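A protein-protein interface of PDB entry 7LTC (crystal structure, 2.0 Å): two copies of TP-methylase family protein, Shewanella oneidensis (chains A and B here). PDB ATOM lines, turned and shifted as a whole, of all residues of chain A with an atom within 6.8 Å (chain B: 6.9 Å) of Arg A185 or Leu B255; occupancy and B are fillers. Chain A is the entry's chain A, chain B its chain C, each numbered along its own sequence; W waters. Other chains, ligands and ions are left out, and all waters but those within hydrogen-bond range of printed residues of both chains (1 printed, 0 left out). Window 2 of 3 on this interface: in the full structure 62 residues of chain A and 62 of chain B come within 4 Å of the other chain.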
ATOM      1  N   SER A 148      23.518  -6.664  -2.684  1.00  0.00           N
ATOM      2  CA  SER A 148      24.867  -6.663  -3.278  1.00  0.00           C
ATOM      3  C   SER A 148      25.922  -6.441  -2.192  1.00  0.00           C
ATOM      4  O   SER A 148      27.042  -6.951  -2.299  1.00  0.00           O
ATOM      5  CB  SER A 148      25.016  -5.646  -4.378  1.00  0.00           C
ATOM      6  OG  SER A 148      24.189  -5.977  -5.483  1.00  0.00           O
ATOM      7  N   MET A 151      26.723  -9.685  -0.673  1.00  0.00           N
ATOM      8  CA  MET A 151      27.565 -10.506  -1.547  1.00  0.00           C
ATOM      9  C   MET A 151      29.001  -9.958  -1.563  1.00  0.00           C
ATOM     10  O   MET A 151      29.956 -10.742  -1.517  1.00  0.00           O
ATOM     11  CB  MET A 151      27.001 -10.546  -2.974  1.00  0.00           C
ATOM     12  CG  MET A 151      25.635 -11.214  -3.073  1.00  0.00           C
ATOM     13  SD  MET A 151      25.039 -11.366  -4.794  1.00  0.00           S
ATOM     14  CE  MET A 151      26.081 -12.664  -5.462  1.00  0.00           C
ATOM     15  N   PHE A 152      29.180  -8.636  -1.585  1.00  0.00           N
ATOM     16  CA  PHE A 152      30.510  -8.045  -1.840  1.00  0.00           C
ATOM     17  C   PHE A 152      31.329  -7.889  -0.553  1.00  0.00           C
ATOM     18  O   PHE A 152      32.557  -7.806  -0.609  1.00  0.00           O
ATOM     19  CB  PHE A 152      30.395  -6.661  -2.484  1.00  0.00           C
ATOM     20  CG  PHE A 152      29.714  -6.616  -3.827  1.00  0.00           C
ATOM     21  CD1 PHE A 152      29.670  -7.734  -4.644  1.00  0.00           C
ATOM     22  CD2 PHE A 152      29.161  -5.432  -4.289  1.00  0.00           C
ATOM     23  CE1 PHE A 152      29.062  -7.672  -5.888  1.00  0.00           C
ATOM     24  CE2 PHE A 152      28.563  -5.371  -5.538  1.00  0.00           C
ATOM     25  CZ  PHE A 152      28.509  -6.493  -6.331  1.00  0.00           C
ATOM     26  N   ALA A 171      21.105  -7.818  -7.330  1.00  0.00           N
ATOM     27  CA  ALA A 171      22.077  -8.509  -6.472  1.00  0.00           C
ATOM     28  C   ALA A 171      23.286  -8.950  -7.308  1.00  0.00           C
ATOM     29  O   ALA A 171      23.166  -9.761  -8.232  1.00  0.00           O
ATOM     30  CB  ALA A 171      21.412  -9.678  -5.786  1.00  0.00           C
ATOM     31  N   GLY A 172      24.444  -8.383  -6.997  1.00  0.00           N
ATOM     32  CA  GLY A 172      25.681  -8.781  -7.648  1.00  0.00           C
ATOM     33  C   GLY A 172      26.017  -7.896  -8.840  1.00  0.00           C
ATOM     34  O   GLY A 172      27.037  -8.112  -9.492  1.00  0.00           O
ATOM     35  N   GLU A 173      25.171  -6.909  -9.134  1.00  0.00           N
ATOM     36  CA  GLU A 173      25.404  -5.994 -10.260  1.00  0.00           C
ATOM     37  C   GLU A 173      26.435  -4.927  -9.854  1.00  0.00           C
ATOM     38  O   GLU A 173      26.067  -3.855  -9.372  1.00  0.00           O
ATOM     39  CB  GLU A 173      24.085  -5.358 -10.703  1.00  0.00           C
ATOM     40  CG  GLU A 173      24.088  -4.949 -12.159  1.00  0.00           C
ATOM     41  CD  GLU A 173      25.105  -3.874 -12.499  1.00  0.00           C
ATOM     42  OE1 GLU A 173      24.772  -2.677 -12.352  1.00  0.00           O
ATOM     43  OE2 GLU A 173      26.227  -4.234 -12.911  1.00  0.00           O
ATOM     44  N   HIS A 174      27.720  -5.207 -10.090  1.00  0.00           N
ATOM     45  CA  HIS A 174      28.824  -4.466  -9.439  1.00  0.00           C
ATOM     46  C   HIS A 174      29.109  -3.134 -10.154  1.00  0.00           C
ATOM     47  O   HIS A 174      29.697  -2.239  -9.550  1.00  0.00           O
ATOM     48  CB  HIS A 174      30.100  -5.328  -9.381  1.00  0.00           C
ATOM     49  CG  HIS A 174      30.678  -5.583 -10.733  1.00  0.00           C
ATOM     50  ND1 HIS A 174      30.239  -6.616 -11.541  1.00  0.00           N
ATOM     51  CD2 HIS A 174      31.613  -4.919 -11.448  1.00  0.00           C
ATOM     52  CE1 HIS A 174      30.897  -6.588 -12.683  1.00  0.00           C
ATOM     53  NE2 HIS A 174      31.742  -5.557 -12.652  1.00  0.00           N
ATOM     54  N   THR A 181      19.997  -7.771 -12.373  1.00  0.00           N
ATOM     55  CA  THR A 181      21.131  -8.720 -12.352  1.00  0.00           C
ATOM     56  C   THR A 181      20.836  -9.875 -13.321  1.00  0.00           C
ATOM     57  O   THR A 181      19.980  -9.755 -14.200  1.00  0.00           O
ATOM     58  CB  THR A 181      21.445  -9.177 -10.918  1.00  0.00           C
ATOM     59  OG1 THR A 181      22.671  -9.913 -10.925  1.00  0.00           O
ATOM     60  CG2 THR A 181      20.355 -10.023 -10.298  1.00  0.00           C
ATOM     61  N   SER A 182      21.565 -10.977 -13.174  1.00  0.00           N
ATOM     62  CA  SER A 182      21.365 -12.158 -14.016  1.00  0.00           C
ATOM     63  C   SER A 182      21.093 -13.387 -13.139  1.00  0.00           C
ATOM     64  O   SER A 182      21.358 -13.379 -11.935  1.00  0.00           O
ATOM     65  CB  SER A 182      22.553 -12.386 -14.916  1.00  0.00           C
ATOM     66  OG  SER A 182      23.682 -12.800 -14.161  1.00  0.00           O
ATOM     67  N   SER A 183      20.564 -14.437 -13.764  1.00  0.00           N
ATOM     68  CA  SER A 183      20.274 -15.712 -13.092  1.00  0.00           C
ATOM     69  C   SER A 183      21.527 -16.289 -12.414  1.00  0.00           C
ATOM     70  O   SER A 183      21.426 -16.842 -11.319  1.00  0.00           O
ATOM     71  CB  SER A 183      19.686 -16.713 -14.057  1.00  0.00           C
ATOM     72  OG  SER A 183      20.673 -17.176 -14.969  1.00  0.00           O
ATOM     73  N   ASP A 184      22.696 -16.189 -13.047  1.00  0.00           N
ATOM     74  CA  ASP A 184      23.912 -16.825 -12.491  1.00  0.00           C
ATOM     75  C   ASP A 184      24.355 -16.115 -11.200  1.00  0.00           C
ATOM     76  O   ASP A 184      24.888 -16.759 -10.295  1.00  0.00           O
ATOM     77  CB  ASP A 184      25.061 -16.848 -13.503  1.00  0.00           C
ATOM     78  CG  ASP A 184      25.493 -15.465 -13.954  1.00  0.00           C
ATOM     79  OD1 ASP A 184      24.647 -14.747 -14.524  1.00  0.00           O
ATOM     80  OD2 ASP A 184      26.668 -15.114 -13.726  1.00  0.00           O
ATOM     81  N   ARG A 185      24.164 -14.799 -11.121  1.00  0.00           N
ATOM     82  CA  ARG A 185      24.511 -14.035  -9.906  1.00  0.00           C
ATOM     83  C   ARG A 185      23.637 -14.490  -8.730  1.00  0.00           C
ATOM     84  O   ARG A 185      24.133 -14.682  -7.618  1.00  0.00           O
ATOM     85  CB  ARG A 185      24.319 -12.527 -10.109  1.00  0.00           C
ATOM     86  CG  ARG A 185      25.130 -11.928 -11.249  1.00  0.00           C
ATOM     87  CD  ARG A 185      26.543 -11.650 -10.793  1.00  0.00           C
ATOM     88  NE  ARG A 185      27.437 -11.216 -11.854  1.00  0.00           N
ATOM     89  CZ  ARG A 185      28.563 -11.840 -12.181  1.00  0.00           C
ATOM     90  NH1 ARG A 185      28.577 -13.154 -12.341  1.00  0.00           N
ATOM     91  NH2 ARG A 185      29.668 -11.138 -12.370  1.00  0.00           N
ATOM     92  N   LEU A 186      22.343 -14.646  -8.988  1.00  0.00           N
ATOM     93  CA  LEU A 186      21.382 -15.072  -7.968  1.00  0.00           C
ATOM     94  C   LEU A 186      21.648 -16.527  -7.545  1.00  0.00           C
ATOM     95  O   LEU A 186      21.428 -16.868  -6.388  1.00  0.00           O
ATOM     96  CB  LEU A 186      19.966 -14.899  -8.523  1.00  0.00           C
ATOM     97  CG  LEU A 186      19.467 -13.458  -8.655  1.00  0.00           C
ATOM     98  CD1 LEU A 186      18.191 -13.437  -9.475  1.00  0.00           C
ATOM     99  CD2 LEU A 186      19.225 -12.793  -7.302  1.00  0.00           C
ATOM    100  N   GLN A 187      22.097 -17.394  -8.454  1.00  0.00           N
ATOM    101  CA  GLN A 187      22.541 -18.751  -8.046  1.00  0.00           C
ATOM    102  C   GLN A 187      23.716 -18.639  -7.060  1.00  0.00           C
ATOM    103  O   GLN A 187      23.792 -19.410  -6.108  1.00  0.00           O
ATOM    104  CB  GLN A 187      22.910 -19.603  -9.267  1.00  0.00           C
ATOM    105  CG  GLN A 187      23.389 -21.018  -8.939  1.00  0.00           C
ATOM    106  CD  GLN A 187      22.418 -21.826  -8.114  1.00  0.00           C
ATOM    107  OE1 GLN A 187      21.201 -21.702  -8.243  1.00  0.00           O
ATOM    108  NE2 GLN A 187      22.958 -22.666  -7.244  1.00  0.00           N
ATOM    109  N   ILE A 188      24.636 -17.699  -7.267  1.00  0.00           N
ATOM    110  CA  ILE A 188      25.786 -17.566  -6.360  1.00  0.00           C
ATOM    111  C   ILE A 188      25.294 -17.108  -4.974  1.00  0.00           C
ATOM    112  O   ILE A 188      25.820 -17.533  -3.939  1.00  0.00           O
ATOM    113  CB  ILE A 188      26.852 -16.631  -6.974  1.00  0.00           C
ATOM    114  CG1 ILE A 188      27.522 -17.276  -8.195  1.00  0.00           C
ATOM    115  CG2 ILE A 188      27.863 -16.209  -5.923  1.00  0.00           C
ATOM    116  CD1 ILE A 188      28.468 -16.377  -8.957  1.00  0.00           C
ATOM    117  N   LEU A 189      24.269 -16.262  -4.955  1.00  0.00           N
ATOM    118  CA  LEU A 189      23.697 -15.775  -3.697  1.00  0.00           C
ATOM    119  C   LEU A 189      23.064 -16.960  -2.964  1.00  0.00           C
ATOM    120  O   LEU A 189      23.192 -17.100  -1.748  1.00  0.00           O
ATOM    121  CB  LEU A 189      22.663 -14.680  -3.993  1.00  0.00           C
ATOM    122  CG  LEU A 189      21.883 -14.150  -2.787  1.00  0.00           C
ATOM    123  CD1 LEU A 189      22.819 -13.583  -1.730  1.00  0.00           C
ATOM    124  CD2 LEU A 189      20.853 -13.104  -3.204  1.00  0.00           C
ATOM    125  N   VAL A 190      22.403 -17.822  -3.725  1.00  0.00           N
ATOM    126  CA  VAL A 190      21.755 -18.993  -3.144  1.00  0.00           C
ATOM    127  C   VAL A 190      22.822 -19.861  -2.465  1.00  0.00           C
ATOM    128  O   VAL A 190      22.626 -20.339  -1.344  1.00  0.00           O
ATOM    129  CB  VAL A 190      20.965 -19.790  -4.202  1.00  0.00           C
ATOM    130  CG1 VAL A 190      20.630 -21.202  -3.741  1.00  0.00           C
ATOM    131  CG2 VAL A 190      19.693 -19.069  -4.615  1.00  0.00           C
ATOM    132  N   PRO A 227      16.768 -18.019  -8.458  1.00  0.00           N
ATOM    133  CA  PRO A 227      17.363 -17.535  -9.720  1.00  0.00           C
ATOM    134  C   PRO A 227      16.408 -17.632 -10.921  1.00  0.00           C
ATOM    135  O   PRO A 227      16.706 -17.069 -11.973  1.00  0.00           O
ATOM    136  CB  PRO A 227      18.603 -18.408  -9.992  1.00  0.00           C
ATOM    137  CG  PRO A 227      18.897 -19.033  -8.655  1.00  0.00           C
ATOM    138  CD  PRO A 227      17.523 -19.208  -8.043  1.00  0.00           C
ATOM    139  N   TYR B 249      36.176 -11.880  -0.385  1.00  0.00           N
ATOM    140  CA  TYR B 249      37.031 -12.332  -1.516  1.00  0.00           C
ATOM    141  C   TYR B 249      36.467 -13.612  -2.155  1.00  0.00           C
ATOM    142  O   TYR B 249      36.494 -13.763  -3.375  1.00  0.00           O
ATOM    143  CB  TYR B 249      38.488 -12.501  -1.060  1.00  0.00           C
ATOM    144  CG  TYR B 249      39.211 -11.196  -0.844  1.00  0.00           C
ATOM    145  CD1 TYR B 249      39.480 -10.367  -1.918  1.00  0.00           C
ATOM    146  CD2 TYR B 249      39.613 -10.774   0.416  1.00  0.00           C
ATOM    147  CE1 TYR B 249      40.124  -9.153  -1.753  1.00  0.00           C
ATOM    148  CE2 TYR B 249      40.266  -9.565   0.596  1.00  0.00           C
ATOM    149  CZ  TYR B 249      40.524  -8.753  -0.493  1.00  0.00           C
ATOM    150  OH  TYR B 249      41.164  -7.557  -0.329  1.00  0.00           O
ATOM    151  N   ALA B 250      35.962 -14.524  -1.336  1.00  0.00           N
ATOM    152  CA  ALA B 250      35.345 -15.773  -1.811  1.00  0.00           C
ATOM    153  C   ALA B 250      34.286 -15.504  -2.891  1.00  0.00           C
ATOM    154  O   ALA B 250      34.306 -16.104  -3.971  1.00  0.00           O
ATOM    155  CB  ALA B 250      34.725 -16.489  -0.637  1.00  0.00           C
ATOM    156  N   ILE B 251      33.337 -14.634  -2.569  1.00  0.00           N
ATOM    157  CA  ILE B 251      32.188 -14.385  -3.439  1.00  0.00           C
ATOM    158  C   ILE B 251      32.651 -13.516  -4.616  1.00  0.00           C
ATOM    159  O   ILE B 251      32.251 -13.752  -5.757  1.00  0.00           O
ATOM    160  CB  ILE B 251      31.034 -13.752  -2.629  1.00  0.00           C
ATOM    161  CG1 ILE B 251      30.600 -14.656  -1.472  1.00  0.00           C
ATOM    162  CG2 ILE B 251      29.853 -13.366  -3.513  1.00  0.00           C
ATOM    163  CD1 ILE B 251      30.157 -16.040  -1.887  1.00  0.00           C
ATOM    164  N   LEU B 252      33.509 -12.533  -4.349  1.00  0.00           N
ATOM    165  CA  LEU B 252      34.004 -11.694  -5.442  1.00  0.00           C
ATOM    166  C   LEU B 252      34.630 -12.606  -6.518  1.00  0.00           C
ATOM    167  O   LEU B 252      34.349 -12.417  -7.703  1.00  0.00           O
ATOM    168  CB  LEU B 252      34.974 -10.623  -4.914  1.00  0.00           C
ATOM    169  CG  LEU B 252      34.360  -9.544  -4.012  1.00  0.00           C
ATOM    170  CD1 LEU B 252      35.437  -8.691  -3.356  1.00  0.00           C
ATOM    171  CD2 LEU B 252      33.388  -8.651  -4.780  1.00  0.00           C
ATOM    172  N   ALA B 253      35.416 -13.624  -6.124  1.00  0.00           N
ATOM    173  CA  ALA B 253      36.088 -14.548  -7.097  1.00  0.00           C
ATOM    174  C   ALA B 253      35.046 -15.312  -7.921  1.00  0.00           C
ATOM    175  O   ALA B 253      35.161 -15.418  -9.144  1.00  0.00           O
ATOM    176  CB  ALA B 253      37.011 -15.527  -6.400  1.00  0.00           C
ATOM    177  N   LYS B 254      34.050 -15.867  -7.241  1.00  0.00           N
ATOM    178  CA  LYS B 254      33.014 -16.622  -7.936  1.00  0.00           C
ATOM    179  C   LYS B 254      32.326 -15.704  -8.950  1.00  0.00           C
ATOM    180  O   LYS B 254      31.947 -16.143 -10.037  1.00  0.00           O
ATOM    181  CB  LYS B 254      31.984 -17.187  -6.955  1.00  0.00           C
ATOM    182  CG  LYS B 254      32.511 -18.265  -6.021  1.00  0.00           C
ATOM    183  CD  LYS B 254      31.649 -18.474  -4.799  1.00  0.00           C
ATOM    184  CE  LYS B 254      32.324 -19.308  -3.732  1.00  0.00           C
ATOM    185  NZ  LYS B 254      32.837 -20.592  -4.267  1.00  0.00           N
ATOM    186  N   LEU B 255      32.161 -14.436  -8.576  1.00  0.00           N
ATOM    187  CA  LEU B 255      31.594 -13.430  -9.479  1.00  0.00           C
ATOM    188  C   LEU B 255      32.629 -13.042 -10.549  1.00  0.00           C
ATOM    189  O   LEU B 255      32.283 -12.380 -11.533  1.00  0.00           O
ATOM    190  CB  LEU B 255      31.164 -12.197  -8.672  1.00  0.00           C
ATOM    191  CG  LEU B 255      29.932 -12.361  -7.780  1.00  0.00           C
ATOM    192  CD1 LEU B 255      29.752 -11.150  -6.873  1.00  0.00           C
ATOM    193  CD2 LEU B 255      28.674 -12.589  -8.602  1.00  0.00           C
ATOM    194  N   GLY B 256      33.891 -13.424 -10.342  1.00  0.00           N
ATOM    195  CA  GLY B 256      34.984 -13.128 -11.283  1.00  0.00           C
ATOM    196  C   GLY B 256      35.395 -11.662 -11.275  1.00  0.00           C
ATOM    197  O   GLY B 256      35.818 -11.132 -12.298  1.00  0.00           O
ATOM    198  N   ILE B 257      35.282 -10.999 -10.129  1.00  0.00           N
ATOM    199  CA  ILE B 257      35.651  -9.582 -10.018  1.00  0.00           C
ATOM    200  C   ILE B 257      36.502  -9.389  -8.760  1.00  0.00           C
ATOM    201  O   ILE B 257      36.662 -10.307  -7.967  1.00  0.00           O
ATOM    202  CB  ILE B 257      34.400  -8.680  -9.968  1.00  0.00           C
ATOM    203  CG1 ILE B 257      33.501  -9.051  -8.781  1.00  0.00           C
ATOM    204  CG2 ILE B 257      33.660  -8.715 -11.296  1.00  0.00           C
ATOM    205  CD1 ILE B 257      32.415  -8.043  -8.445  1.00  0.00           C
ATOM    206  N   GLY B 258      37.008  -8.173  -8.593  1.00  0.00           N
ATOM    207  CA  GLY B 258      37.701  -7.740  -7.381  1.00  0.00           C
ATOM    208  C   GLY B 258      37.269  -6.333  -6.998  1.00  0.00           C
ATOM    209  O   GLY B 258      36.520  -5.689  -7.748  1.00  0.00           O
HETATM  210  O   HOH W   1      30.286 -16.172 -12.137  1.00  0.00           O
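Among the printed residues, merely in contact across the chains: Met A151 with Ile B251 (3.3 Å), Phe A152 with Leu B252 (3.8 Å), Phe A152 with Leu B255 (3.7 Å), His A174 with Ile B257 (3.7 Å), Ile A188 with Lys B254 (3.7 Å) and Ile A188 with Leu B255 (3.8 Å).
Water W1 lies within hydrogen-bond range of O of Lys B254 (2.7 Å) and NH1 of Arg A185 (3.5 Å).
No position is printed for both chains.
Of the 10 printed residues of chain B, 5 touch a printed residue of chain A.
Hydrophobic or aromatic side chains of chain B within 4 Å of the printed part of chain A: Ile B251, Leu B252, Leu B255 and Ile B257.
Of the 18 printed residues of chain A, 5 touch a printed residue of chain B.
Hydrophobic or aromatic side chains of chain A that line the printed part of chain B: Phe A152, His A174 and Ile A188.
Among the printed residues, no Asp or Glu carboxylate lies within 4 Å of a Lys or Arg side-chain nitrogen of the other chain.
SD of Met A151 sits at hydrogen-bond distance from N of Gly A172.
O of Leu B252 sits at hydrogen-bond distance from N of Ile B257 (3.0 Å).
OD2 of Asp A184 is in salt-bridge range of NH1 of Arg A185, at 3.1 Å.
Of the printed residues of chain B, Phe A152 touches Leu B252 (3.8 Å) and Leu B255 (3.7 Å).
Leu A186 touches none of the printed residues of chain B.
Printed residues of chain B within 4 Å of Ile A188: Lys B254 (3.7 Å) and Leu B255 (3.8 Å).
Leu B255 touches just these residues of chain A: Phe A152 (3.7 Å), Arg A185 (3.0 Å) and Ile A188 (3.8 Å).
Of the printed residues of chain A, Ile B257 touches His A174 (3.7 Å).
The nearest residue of chain B that does not touch Arg A185 is Ile B257 (4.8 Å).
The guanidinium group of Arg A185 lies within hydrogen-bond range of the backbone carbonyl oxygen of Leu B255, at 3.0 Å.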
